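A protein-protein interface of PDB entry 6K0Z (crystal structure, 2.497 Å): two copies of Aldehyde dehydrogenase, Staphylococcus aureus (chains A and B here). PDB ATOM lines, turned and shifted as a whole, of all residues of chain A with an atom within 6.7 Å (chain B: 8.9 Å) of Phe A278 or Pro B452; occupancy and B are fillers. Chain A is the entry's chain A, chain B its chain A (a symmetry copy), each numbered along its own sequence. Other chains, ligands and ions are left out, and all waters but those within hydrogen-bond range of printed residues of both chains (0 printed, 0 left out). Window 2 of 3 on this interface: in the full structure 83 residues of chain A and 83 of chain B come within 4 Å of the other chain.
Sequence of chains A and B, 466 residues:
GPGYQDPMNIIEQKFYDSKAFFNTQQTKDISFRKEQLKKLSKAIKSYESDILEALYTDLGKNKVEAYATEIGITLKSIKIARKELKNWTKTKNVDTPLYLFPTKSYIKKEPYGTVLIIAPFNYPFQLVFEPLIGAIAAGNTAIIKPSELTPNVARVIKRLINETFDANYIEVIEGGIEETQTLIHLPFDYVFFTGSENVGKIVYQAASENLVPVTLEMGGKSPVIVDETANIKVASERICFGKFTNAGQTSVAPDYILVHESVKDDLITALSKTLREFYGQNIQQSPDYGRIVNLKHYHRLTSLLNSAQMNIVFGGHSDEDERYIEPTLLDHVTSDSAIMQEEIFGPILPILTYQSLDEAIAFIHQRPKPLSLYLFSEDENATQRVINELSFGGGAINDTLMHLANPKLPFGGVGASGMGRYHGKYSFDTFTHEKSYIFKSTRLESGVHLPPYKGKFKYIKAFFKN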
ATOM      1  N   SER A 236     -11.411  15.087   3.760  1.00  0.00           N
ATOM      2  CA  SER A 236     -12.277  13.936   3.737  1.00  0.00           C
ATOM      3  C   SER A 236     -12.480  13.425   2.331  1.00  0.00           C
ATOM      4  O   SER A 236     -12.494  12.231   2.097  1.00  0.00           O
ATOM      5  CB  SER A 236     -13.607  14.293   4.363  1.00  0.00           C
ATOM      6  OG  SER A 236     -14.369  15.086   3.476  1.00  0.00           O
ATOM      7  N   GLU A 237     -12.656  14.351   1.405  1.00  0.00           N
ATOM      8  CA  GLU A 237     -12.852  14.042   0.012  1.00  0.00           C
ATOM      9  C   GLU A 237     -11.548  13.546  -0.580  1.00  0.00           C
ATOM     10  O   GLU A 237     -11.490  12.480  -1.144  1.00  0.00           O
ATOM     11  CB  GLU A 237     -13.295  15.300  -0.732  1.00  0.00           C
ATOM     12  CG  GLU A 237     -14.754  15.680  -0.551  1.00  0.00           C
ATOM     13  CD  GLU A 237     -15.015  17.153  -0.788  1.00  0.00           C
ATOM     14  OE1 GLU A 237     -14.078  17.916  -1.063  1.00  0.00           O
ATOM     15  OE2 GLU A 237     -16.171  17.547  -0.696  1.00  0.00           O
ATOM     16  N   ARG A 238     -10.497  14.332  -0.427  1.00  0.00           N
ATOM     17  CA  ARG A 238      -9.193  13.967  -0.937  1.00  0.00           C
ATOM     18  C   ARG A 238      -8.738  12.581  -0.480  1.00  0.00           C
ATOM     19  O   ARG A 238      -8.299  11.801  -1.271  1.00  0.00           O
ATOM     20  CB  ARG A 238      -8.167  15.042  -0.608  1.00  0.00           C
ATOM     21  CG  ARG A 238      -8.204  16.206  -1.568  1.00  0.00           C
ATOM     22  CD  ARG A 238      -7.235  17.320  -1.242  1.00  0.00           C
ATOM     23  NE  ARG A 238      -7.660  18.566  -1.862  1.00  0.00           N
ATOM     24  CZ  ARG A 238      -6.989  19.710  -1.819  1.00  0.00           C
ATOM     25  NH1 ARG A 238      -5.844  19.811  -1.190  1.00  0.00           N
ATOM     26  NH2 ARG A 238      -7.469  20.769  -2.417  1.00  0.00           N
ATOM     27  N   ILE A 239      -8.906  12.256   0.786  1.00  0.00           N
ATOM     28  CA  ILE A 239      -8.517  10.966   1.305  1.00  0.00           C
ATOM     29  C   ILE A 239      -9.350   9.886   0.692  1.00  0.00           C
ATOM     30  O   ILE A 239      -8.868   8.827   0.377  1.00  0.00           O
ATOM     31  CB  ILE A 239      -8.720  10.872   2.828  1.00  0.00           C
ATOM     32  CG1 ILE A 239      -7.586  11.531   3.573  1.00  0.00           C
ATOM     33  CG2 ILE A 239      -8.834   9.436   3.277  1.00  0.00           C
ATOM     34  CD1 ILE A 239      -7.877  11.721   5.028  1.00  0.00           C
ATOM     35  N   CYS A 240     -10.622  10.140   0.509  1.00  0.00           N
ATOM     36  CA  CYS A 240     -11.478   9.122  -0.026  1.00  0.00           C
ATOM     37  C   CYS A 240     -11.279   8.858  -1.500  1.00  0.00           C
ATOM     38  O   CYS A 240     -11.617   7.804  -1.992  1.00  0.00           O
ATOM     39  CB  CYS A 240     -12.900   9.484   0.261  1.00  0.00           C
ATOM     40  SG  CYS A 240     -13.609   8.460   1.526  1.00  0.00           S
ATOM     41  N   PHE A 241     -10.759   9.830  -2.217  1.00  0.00           N
ATOM     42  CA  PHE A 241     -10.491   9.620  -3.592  1.00  0.00           C
ATOM     43  C   PHE A 241      -9.379   8.595  -3.606  1.00  0.00           C
ATOM     44  O   PHE A 241      -9.514   7.526  -4.162  1.00  0.00           O
ATOM     45  CB  PHE A 241     -10.044  10.910  -4.236  1.00  0.00           C
ATOM     46  CG  PHE A 241      -9.542  10.730  -5.611  1.00  0.00           C
ATOM     47  CD1 PHE A 241     -10.194   9.905  -6.470  1.00  0.00           C
ATOM     48  CD2 PHE A 241      -8.411  11.346  -6.019  1.00  0.00           C
ATOM     49  CE1 PHE A 241      -9.728   9.701  -7.730  1.00  0.00           C
ATOM     50  CE2 PHE A 241      -7.929  11.149  -7.281  1.00  0.00           C
ATOM     51  CZ  PHE A 241      -8.591  10.329  -8.139  1.00  0.00           C
ATOM     52  N   GLY A 242      -8.289   8.929  -2.934  1.00  0.00           N
ATOM     53  CA  GLY A 242      -7.140   8.065  -2.814  1.00  0.00           C
ATOM     54  C   GLY A 242      -7.473   6.681  -2.330  1.00  0.00           C
ATOM     55  O   GLY A 242      -7.025   5.705  -2.893  1.00  0.00           O
ATOM     56  N   PHE A 244     -10.638   5.210  -2.033  1.00  0.00           N
ATOM     57  CA  PHE A 244     -11.707   4.480  -2.666  1.00  0.00           C
ATOM     58  C   PHE A 244     -11.711   4.278  -4.175  1.00  0.00           C
ATOM     59  O   PHE A 244     -12.576   3.640  -4.721  1.00  0.00           O
ATOM     60  CB  PHE A 244     -13.021   4.866  -2.045  1.00  0.00           C
ATOM     61  CG  PHE A 244     -13.149   4.380  -0.657  1.00  0.00           C
ATOM     62  CD1 PHE A 244     -13.374   3.064  -0.413  1.00  0.00           C
ATOM     63  CD2 PHE A 244     -12.980   5.218   0.389  1.00  0.00           C
ATOM     64  CE1 PHE A 244     -13.479   2.598   0.862  1.00  0.00           C
ATOM     65  CE2 PHE A 244     -13.085   4.768   1.669  1.00  0.00           C
ATOM     66  CZ  PHE A 244     -13.332   3.456   1.904  1.00  0.00           C
ATOM     67  N   LYS A 273     -20.069  11.619   5.256  1.00  0.00           N
ATOM     68  CA  LYS A 273     -20.856  12.571   4.508  1.00  0.00           C
ATOM     69  C   LYS A 273     -20.268  12.796   3.128  1.00  0.00           C
ATOM     70  O   LYS A 273     -20.980  12.758   2.147  1.00  0.00           O
ATOM     71  CB  LYS A 273     -21.017  13.867   5.275  1.00  0.00           C
ATOM     72  CG  LYS A 273     -22.208  13.836   6.214  1.00  0.00           C
ATOM     73  CD  LYS A 273     -22.587  12.419   6.584  1.00  0.00           C
ATOM     74  CE  LYS A 273     -23.095  12.347   8.018  1.00  0.00           C
ATOM     75  NZ  LYS A 273     -23.549  10.981   8.393  1.00  0.00           N
ATOM     76  N   THR A 274     -18.959  12.980   3.029  1.00  0.00           N
ATOM     77  CA  THR A 274     -18.387  13.180   1.719  1.00  0.00           C
ATOM     78  C   THR A 274     -18.118  11.876   1.032  1.00  0.00           C
ATOM     79  O   THR A 274     -17.471  11.855   0.027  1.00  0.00           O
ATOM     80  CB  THR A 274     -17.132  14.041   1.711  1.00  0.00           C
ATOM     81  OG1 THR A 274     -16.210  13.522   2.648  1.00  0.00           O
ATOM     82  CG2 THR A 274     -17.457  15.443   2.091  1.00  0.00           C
ATOM     83  N   LEU A 275     -18.561  10.785   1.617  1.00  0.00           N
ATOM     84  CA  LEU A 275     -18.484   9.496   0.952  1.00  0.00           C
ATOM     85  C   LEU A 275     -19.788   9.321   0.197  1.00  0.00           C
ATOM     86  O   LEU A 275     -19.843   8.628  -0.791  1.00  0.00           O
ATOM     87  CB  LEU A 275     -18.349   8.352   1.938  1.00  0.00           C
ATOM     88  CG  LEU A 275     -17.077   7.503   1.987  1.00  0.00           C
ATOM     89  CD1 LEU A 275     -16.475   7.664   3.352  1.00  0.00           C
ATOM     90  CD2 LEU A 275     -17.392   6.044   1.802  1.00  0.00           C
ATOM     91  N   ARG A 276     -20.849   9.967   0.687  1.00  0.00           N
ATOM     92  CA  ARG A 276     -22.175   9.964   0.094  1.00  0.00           C
ATOM     93  C   ARG A 276     -22.143  10.915  -1.085  1.00  0.00           C
ATOM     94  O   ARG A 276     -22.806  10.719  -2.053  1.00  0.00           O
ATOM     95  CB  ARG A 276     -23.195  10.378   1.129  1.00  0.00           C
ATOM     96  CG  ARG A 276     -23.376   9.364   2.237  1.00  0.00           C
ATOM     97  CD  ARG A 276     -23.658   7.977   1.713  1.00  0.00           C
ATOM     98  NE  ARG A 276     -24.103   7.105   2.790  1.00  0.00           N
ATOM     99  CZ  ARG A 276     -24.386   5.818   2.649  1.00  0.00           C
ATOM    100  NH1 ARG A 276     -24.266   5.241   1.473  1.00  0.00           N
ATOM    101  NH2 ARG A 276     -24.787   5.107   3.681  1.00  0.00           N
ATOM    102  N   GLU A 277     -21.317  11.929  -0.960  1.00  0.00           N
ATOM    103  CA  GLU A 277     -21.093  12.859  -2.027  1.00  0.00           C
ATOM    104  C   GLU A 277     -20.375  12.157  -3.170  1.00  0.00           C
ATOM    105  O   GLU A 277     -20.255  12.702  -4.258  1.00  0.00           O
ATOM    106  CB  GLU A 277     -20.137  13.934  -1.558  1.00  0.00           C
ATOM    107  CG  GLU A 277     -20.693  14.941  -0.597  1.00  0.00           C
ATOM    108  CD  GLU A 277     -20.161  16.315  -0.886  1.00  0.00           C
ATOM    109  OE1 GLU A 277     -19.057  16.644  -0.438  1.00  0.00           O
ATOM    110  OE2 GLU A 277     -20.852  17.067  -1.575  1.00  0.00           O
ATOM    111  N   PHE A 278     -19.854  10.967  -2.915  1.00  0.00           N
ATOM    112  CA  PHE A 278     -19.112  10.250  -3.908  1.00  0.00           C
ATOM    113  C   PHE A 278     -19.932   9.150  -4.515  1.00  0.00           C
ATOM    114  O   PHE A 278     -20.021   9.064  -5.718  1.00  0.00           O
ATOM    115  CB  PHE A 278     -17.888   9.620  -3.272  1.00  0.00           C
ATOM    116  CG  PHE A 278     -16.729  10.521  -3.142  1.00  0.00           C
ATOM    117  CD1 PHE A 278     -16.887  11.855  -3.136  1.00  0.00           C
ATOM    118  CD2 PHE A 278     -15.482  10.010  -3.022  1.00  0.00           C
ATOM    119  CE1 PHE A 278     -15.805  12.688  -3.014  1.00  0.00           C
ATOM    120  CE2 PHE A 278     -14.398  10.821  -2.893  1.00  0.00           C
ATOM    121  CZ  PHE A 278     -14.555  12.165  -2.894  1.00  0.00           C
ATOM    122  N   TYR A 279     -20.507   8.295  -3.686  1.00  0.00           N
ATOM    123  CA  TYR A 279     -21.274   7.176  -4.201  1.00  0.00           C
ATOM    124  C   TYR A 279     -22.693   7.050  -3.698  1.00  0.00           C
ATOM    125  O   TYR A 279     -23.263   5.990  -3.828  1.00  0.00           O
ATOM    126  CB  TYR A 279     -20.565   5.853  -3.912  1.00  0.00           C
ATOM    127  CG  TYR A 279     -19.066   5.896  -4.048  1.00  0.00           C
ATOM    128  CD1 TYR A 279     -18.446   5.552  -5.228  1.00  0.00           C
ATOM    129  CD2 TYR A 279     -18.274   6.265  -2.987  1.00  0.00           C
ATOM    130  CE1 TYR A 279     -17.082   5.600  -5.349  1.00  0.00           C
ATOM    131  CE2 TYR A 279     -16.910   6.320  -3.105  1.00  0.00           C
ATOM    132  CZ  TYR A 279     -16.323   5.975  -4.285  1.00  0.00           C
ATOM    133  OH  TYR A 279     -14.976   6.030  -4.404  1.00  0.00           O
ATOM    134  N   GLY A 280     -23.239   8.098  -3.080  1.00  0.00           N
ATOM    135  CA  GLY A 280     -24.613   8.130  -2.581  1.00  0.00           C
ATOM    136  C   GLY A 280     -25.090   7.120  -1.570  1.00  0.00           C
ATOM    137  O   GLY A 280     -24.310   6.393  -1.010  1.00  0.00           O
ATOM    138  N   ILE A 283     -24.075   2.233  -2.095  1.00  0.00           N
ATOM    139  CA  ILE A 283     -22.924   2.287  -2.954  1.00  0.00           C
ATOM    140  C   ILE A 283     -22.870   1.088  -3.870  1.00  0.00           C
ATOM    141  O   ILE A 283     -22.302   1.152  -4.923  1.00  0.00           O
ATOM    142  CB  ILE A 283     -21.679   2.363  -2.080  1.00  0.00           C
ATOM    143  CG1 ILE A 283     -21.928   3.306  -0.930  1.00  0.00           C
ATOM    144  CG2 ILE A 283     -20.479   2.811  -2.871  1.00  0.00           C
ATOM    145  CD1 ILE A 283     -21.149   4.576  -1.027  1.00  0.00           C
ATOM    146  N   SER A 286     -23.497   1.957  -7.169  1.00  0.00           N
ATOM    147  CA  SER A 286     -22.888   3.107  -7.829  1.00  0.00           C
ATOM    148  C   SER A 286     -22.027   2.666  -9.009  1.00  0.00           C
ATOM    149  O   SER A 286     -21.269   1.696  -8.901  1.00  0.00           O
ATOM    150  CB  SER A 286     -22.026   3.905  -6.857  1.00  0.00           C
ATOM    151  OG  SER A 286     -21.278   4.893  -7.548  1.00  0.00           O
ATOM    152  N   ASP A 288     -19.515   4.276  -9.941  1.00  0.00           N
ATOM    153  CA  ASP A 288     -18.311   5.066  -9.727  1.00  0.00           C
ATOM    154  C   ASP A 288     -17.341   4.341  -8.813  1.00  0.00           C
ATOM    155  O   ASP A 288     -16.366   4.954  -8.364  1.00  0.00           O
ATOM    156  CB  ASP A 288     -18.650   6.433  -9.134  1.00  0.00           C
ATOM    157  CG  ASP A 288     -19.463   7.287 -10.072  1.00  0.00           C
ATOM    158  OD1 ASP A 288     -18.928   7.662 -11.133  1.00  0.00           O
ATOM    159  OD2 ASP A 288     -20.623   7.602  -9.738  1.00  0.00           O
ATOM    160  N   SER B 446     -11.877  21.885  -5.418  1.00  0.00           N
ATOM    161  CA  SER B 446     -12.606  21.734  -6.668  1.00  0.00           C
ATOM    162  C   SER B 446     -13.499  20.521  -6.722  1.00  0.00           C
ATOM    163  O   SER B 446     -14.386  20.372  -5.906  1.00  0.00           O
ATOM    164  CB  SER B 446     -11.619  21.701  -7.828  1.00  0.00           C
ATOM    165  OG  SER B 446     -11.838  22.768  -8.729  1.00  0.00           O
ATOM    166  N   GLY B 447     -13.287  19.673  -7.710  1.00  0.00           N
ATOM    167  CA  GLY B 447     -14.070  18.472  -7.865  1.00  0.00           C
ATOM    168  C   GLY B 447     -13.966  17.971  -9.279  1.00  0.00           C
ATOM    169  O   GLY B 447     -14.757  17.153  -9.693  1.00  0.00           O
ATOM    170  N   VAL B 448     -12.963  18.427 -10.011  1.00  0.00           N
ATOM    171  CA  VAL B 448     -12.826  18.048 -11.402  1.00  0.00           C
ATOM    172  C   VAL B 448     -12.534  16.590 -11.693  1.00  0.00           C
ATOM    173  O   VAL B 448     -12.828  16.120 -12.774  1.00  0.00           O
ATOM    174  CB  VAL B 448     -11.816  18.934 -12.118  1.00  0.00           C
ATOM    175  CG1 VAL B 448     -10.781  19.417 -11.145  1.00  0.00           C
ATOM    176  CG2 VAL B 448     -11.172  18.198 -13.269  1.00  0.00           C
ATOM    177  N   HIS B 449     -11.958  15.872 -10.734  1.00  0.00           N
ATOM    178  CA  HIS B 449     -11.659  14.479 -10.956  1.00  0.00           C
ATOM    179  C   HIS B 449     -12.284  13.570  -9.945  1.00  0.00           C
ATOM    180  O   HIS B 449     -12.140  12.370 -10.025  1.00  0.00           O
ATOM    181  CB  HIS B 449     -10.177  14.263 -10.990  1.00  0.00           C
ATOM    182  CG  HIS B 449      -9.474  14.777  -9.792  1.00  0.00           C
ATOM    183  ND1 HIS B 449      -8.644  15.868  -9.837  1.00  0.00           N
ATOM    184  CD2 HIS B 449      -9.458  14.341  -8.517  1.00  0.00           C
ATOM    185  CE1 HIS B 449      -8.150  16.090  -8.636  1.00  0.00           C
ATOM    186  NE2 HIS B 449      -8.633  15.179  -7.817  1.00  0.00           N
ATOM    187  N   LEU B 450     -13.046  14.133  -9.027  1.00  0.00           N
ATOM    188  CA  LEU B 450     -13.665  13.332  -7.999  1.00  0.00           C
ATOM    189  C   LEU B 450     -14.943  12.742  -8.471  1.00  0.00           C
ATOM    190  O   LEU B 450     -15.424  13.099  -9.503  1.00  0.00           O
ATOM    191  CB  LEU B 450     -13.964  14.203  -6.812  1.00  0.00           C
ATOM    192  CG  LEU B 450     -12.732  14.669  -6.079  1.00  0.00           C
ATOM    193  CD1 LEU B 450     -11.731  13.547  -6.118  1.00  0.00           C
ATOM    194  CD2 LEU B 450     -12.154  15.893  -6.721  1.00  0.00           C
ATOM    195  N   PRO B 451     -15.511  11.819  -7.722  1.00  0.00           N
ATOM    196  CA  PRO B 451     -16.797  11.281  -8.136  1.00  0.00           C
ATOM    197  C   PRO B 451     -17.969  12.207  -7.734  1.00  0.00           C
ATOM    198  O   PRO B 451     -17.766  13.175  -7.008  1.00  0.00           O
ATOM    199  CB  PRO B 451     -16.871   9.958  -7.389  1.00  0.00           C
ATOM    200  CG  PRO B 451     -15.478   9.617  -7.083  1.00  0.00           C
ATOM    201  CD  PRO B 451     -14.830  10.924  -6.797  1.00  0.00           C
ATOM    202  N   PRO B 452     -19.197  11.925  -8.209  1.00  0.00           N
ATOM    203  CA  PRO B 452     -19.645  10.872  -9.119  1.00  0.00           C
ATOM    204  C   PRO B 452     -19.220  11.223 -10.506  1.00  0.00           C
ATOM    205  O   PRO B 452     -18.949  12.365 -10.789  1.00  0.00           O
ATOM    206  CB  PRO B 452     -21.156  10.903  -8.973  1.00  0.00           C
ATOM    207  CG  PRO B 452     -21.413  11.659  -7.719  1.00  0.00           C
ATOM    208  CD  PRO B 452     -20.342  12.697  -7.728  1.00  0.00           C
ATOM    209  N   TYR B 453     -19.119  10.241 -11.370  1.00  0.00           N
ATOM    210  CA  TYR B 453     -18.615  10.568 -12.685  1.00  0.00           C
ATOM    211  C   TYR B 453     -19.652  11.035 -13.691  1.00  0.00           C
ATOM    212  O   TYR B 453     -19.337  11.842 -14.543  1.00  0.00           O
ATOM    213  CB  TYR B 453     -17.630   9.509 -13.158  1.00  0.00           C
ATOM    214  CG  TYR B 453     -16.368   9.556 -12.334  1.00  0.00           C
ATOM    215  CD1 TYR B 453     -15.633  10.698 -12.267  1.00  0.00           C
ATOM    216  CD2 TYR B 453     -15.953   8.480 -11.591  1.00  0.00           C
ATOM    217  CE1 TYR B 453     -14.498  10.766 -11.519  1.00  0.00           C
ATOM    218  CE2 TYR B 453     -14.821   8.543 -10.829  1.00  0.00           C
ATOM    219  CZ  TYR B 453     -14.101   9.690 -10.807  1.00  0.00           C
ATOM    220  OH  TYR B 453     -12.971   9.785 -10.067  1.00  0.00           O
ATOM    221  N   LYS B 454     -20.883  10.555 -13.547  1.00  0.00           N
ATOM    222  CA  LYS B 454     -22.043  10.981 -14.350  1.00  0.00           C
ATOM    223  C   LYS B 454     -21.839  11.412 -15.781  1.00  0.00           C
ATOM    224  O   LYS B 454     -22.165  10.691 -16.688  1.00  0.00           O
ATOM    225  CB  LYS B 454     -22.733  12.144 -13.651  1.00  0.00           C
ATOM    226  N   GLY B 455     -21.339  12.623 -15.955  1.00  0.00           N
ATOM    227  CA  GLY B 455     -21.079  13.161 -17.260  1.00  0.00           C
ATOM    228  C   GLY B 455     -19.746  13.844 -17.290  1.00  0.00           C
ATOM    229  O   GLY B 455     -19.586  14.853 -17.934  1.00  0.00           O
ATOM    230  N   LYS B 456     -18.764  13.281 -16.602  1.00  0.00           N
ATOM    231  CA  LYS B 456     -17.468  13.934 -16.543  1.00  0.00           C
ATOM    232  C   LYS B 456     -16.439  13.375 -17.484  1.00  0.00           C
ATOM    233  O   LYS B 456     -15.420  14.012 -17.721  1.00  0.00           O
ATOM    234  CB  LYS B 456     -16.924  13.886 -15.126  1.00  0.00           C
ATOM    235  CG  LYS B 456     -17.758  14.610 -14.099  1.00  0.00           C
ATOM    236  CD  LYS B 456     -16.844  15.274 -13.098  1.00  0.00           C
ATOM    237  CE  LYS B 456     -17.206  14.905 -11.679  1.00  0.00           C
ATOM    238  NZ  LYS B 456     -16.109  15.242 -10.736  1.00  0.00           N
ATOM    239  N   PHE B 457     -16.738  12.200 -18.025  1.00  0.00           N
ATOM    240  CA  PHE B 457     -15.884  11.456 -18.952  1.00  0.00           C
ATOM    241  C   PHE B 457     -15.088  12.290 -19.919  1.00  0.00           C
ATOM    242  O   PHE B 457     -13.886  12.225 -19.953  1.00  0.00           O
ATOM    243  CB  PHE B 457     -16.723  10.483 -19.732  1.00  0.00           C
ATOM    244  CG  PHE B 457     -15.948   9.410 -20.384  1.00  0.00           C
ATOM    245  CD1 PHE B 457     -14.826   9.704 -21.103  1.00  0.00           C
ATOM    246  CD2 PHE B 457     -16.349   8.113 -20.277  1.00  0.00           C
ATOM    247  CE1 PHE B 457     -14.107   8.714 -21.707  1.00  0.00           C
ATOM    248  CE2 PHE B 457     -15.636   7.112 -20.872  1.00  0.00           C
ATOM    249  CZ  PHE B 457     -14.514   7.414 -21.594  1.00  0.00           C
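The side-chain carboxylate (OD1) of Asp A288 lies within hydrogen-bond range of the backbone NH (N) of Tyr B453, at 2.6 Å.
The backbone carbonyl oxygen of His B449 sits at hydrogen-bond distance from the side-chain hydroxyl of Tyr B453 (2.7 Å). The backbone carbonyl oxygen of Leu B450 is in hydrogen-bond range of the side-chain amino group of Lys B456. The side-chain hydroxyl (OG) of Ser A286 is in hydrogen-bond range of the backbone NH (N) of Asp A288 (3.0 Å).
Among the printed residues, merely in contact across the chains: Phe A241 with His B449 (3.7 Å), Phe A241 with Leu B450 (3.6 Å), Phe A241 with Tyr B453 (3.998 Å), Glu A277 with Pro B451 (3.7 Å), Glu A277 with Pro B452 (3.5 Å), Phe A278 with Pro B451 (3.7 Å), Phe A278 with Pro B452 (3.6 Å) and Asp A288 with Pro B452 (3.4 Å).
Of the printed residues of chain B, Phe A241 touches His B449 (3.7 Å), Leu B450 (3.6 Å) and Tyr B453 (3.998 Å). Printed residues of chain B within 4 Å of Glu A277: Pro B451 (3.7 Å) and Pro B452 (3.5 Å). Phe A278 touches two residues of chain B. No residue of chain B comes within 4 Å of Tyr A279. Of the printed residues of chain A, His B449 touches Phe A241. Of the printed residues of chain A, Leu B450 touches Phe A241 (3.6 Å). Pro B452 touches three residues of chain A. Printed residues of chain A within 4 Å of Tyr B453: Phe A241 (3.998 Å) and Asp A288 (2.6 Å).
Hydrophobic or aromatic side chains of chain B within 4 Å of the printed part of chain A: His B449, Leu B450, Pro B451, Pro B452 and Tyr B453.
No position is printed for both chains.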
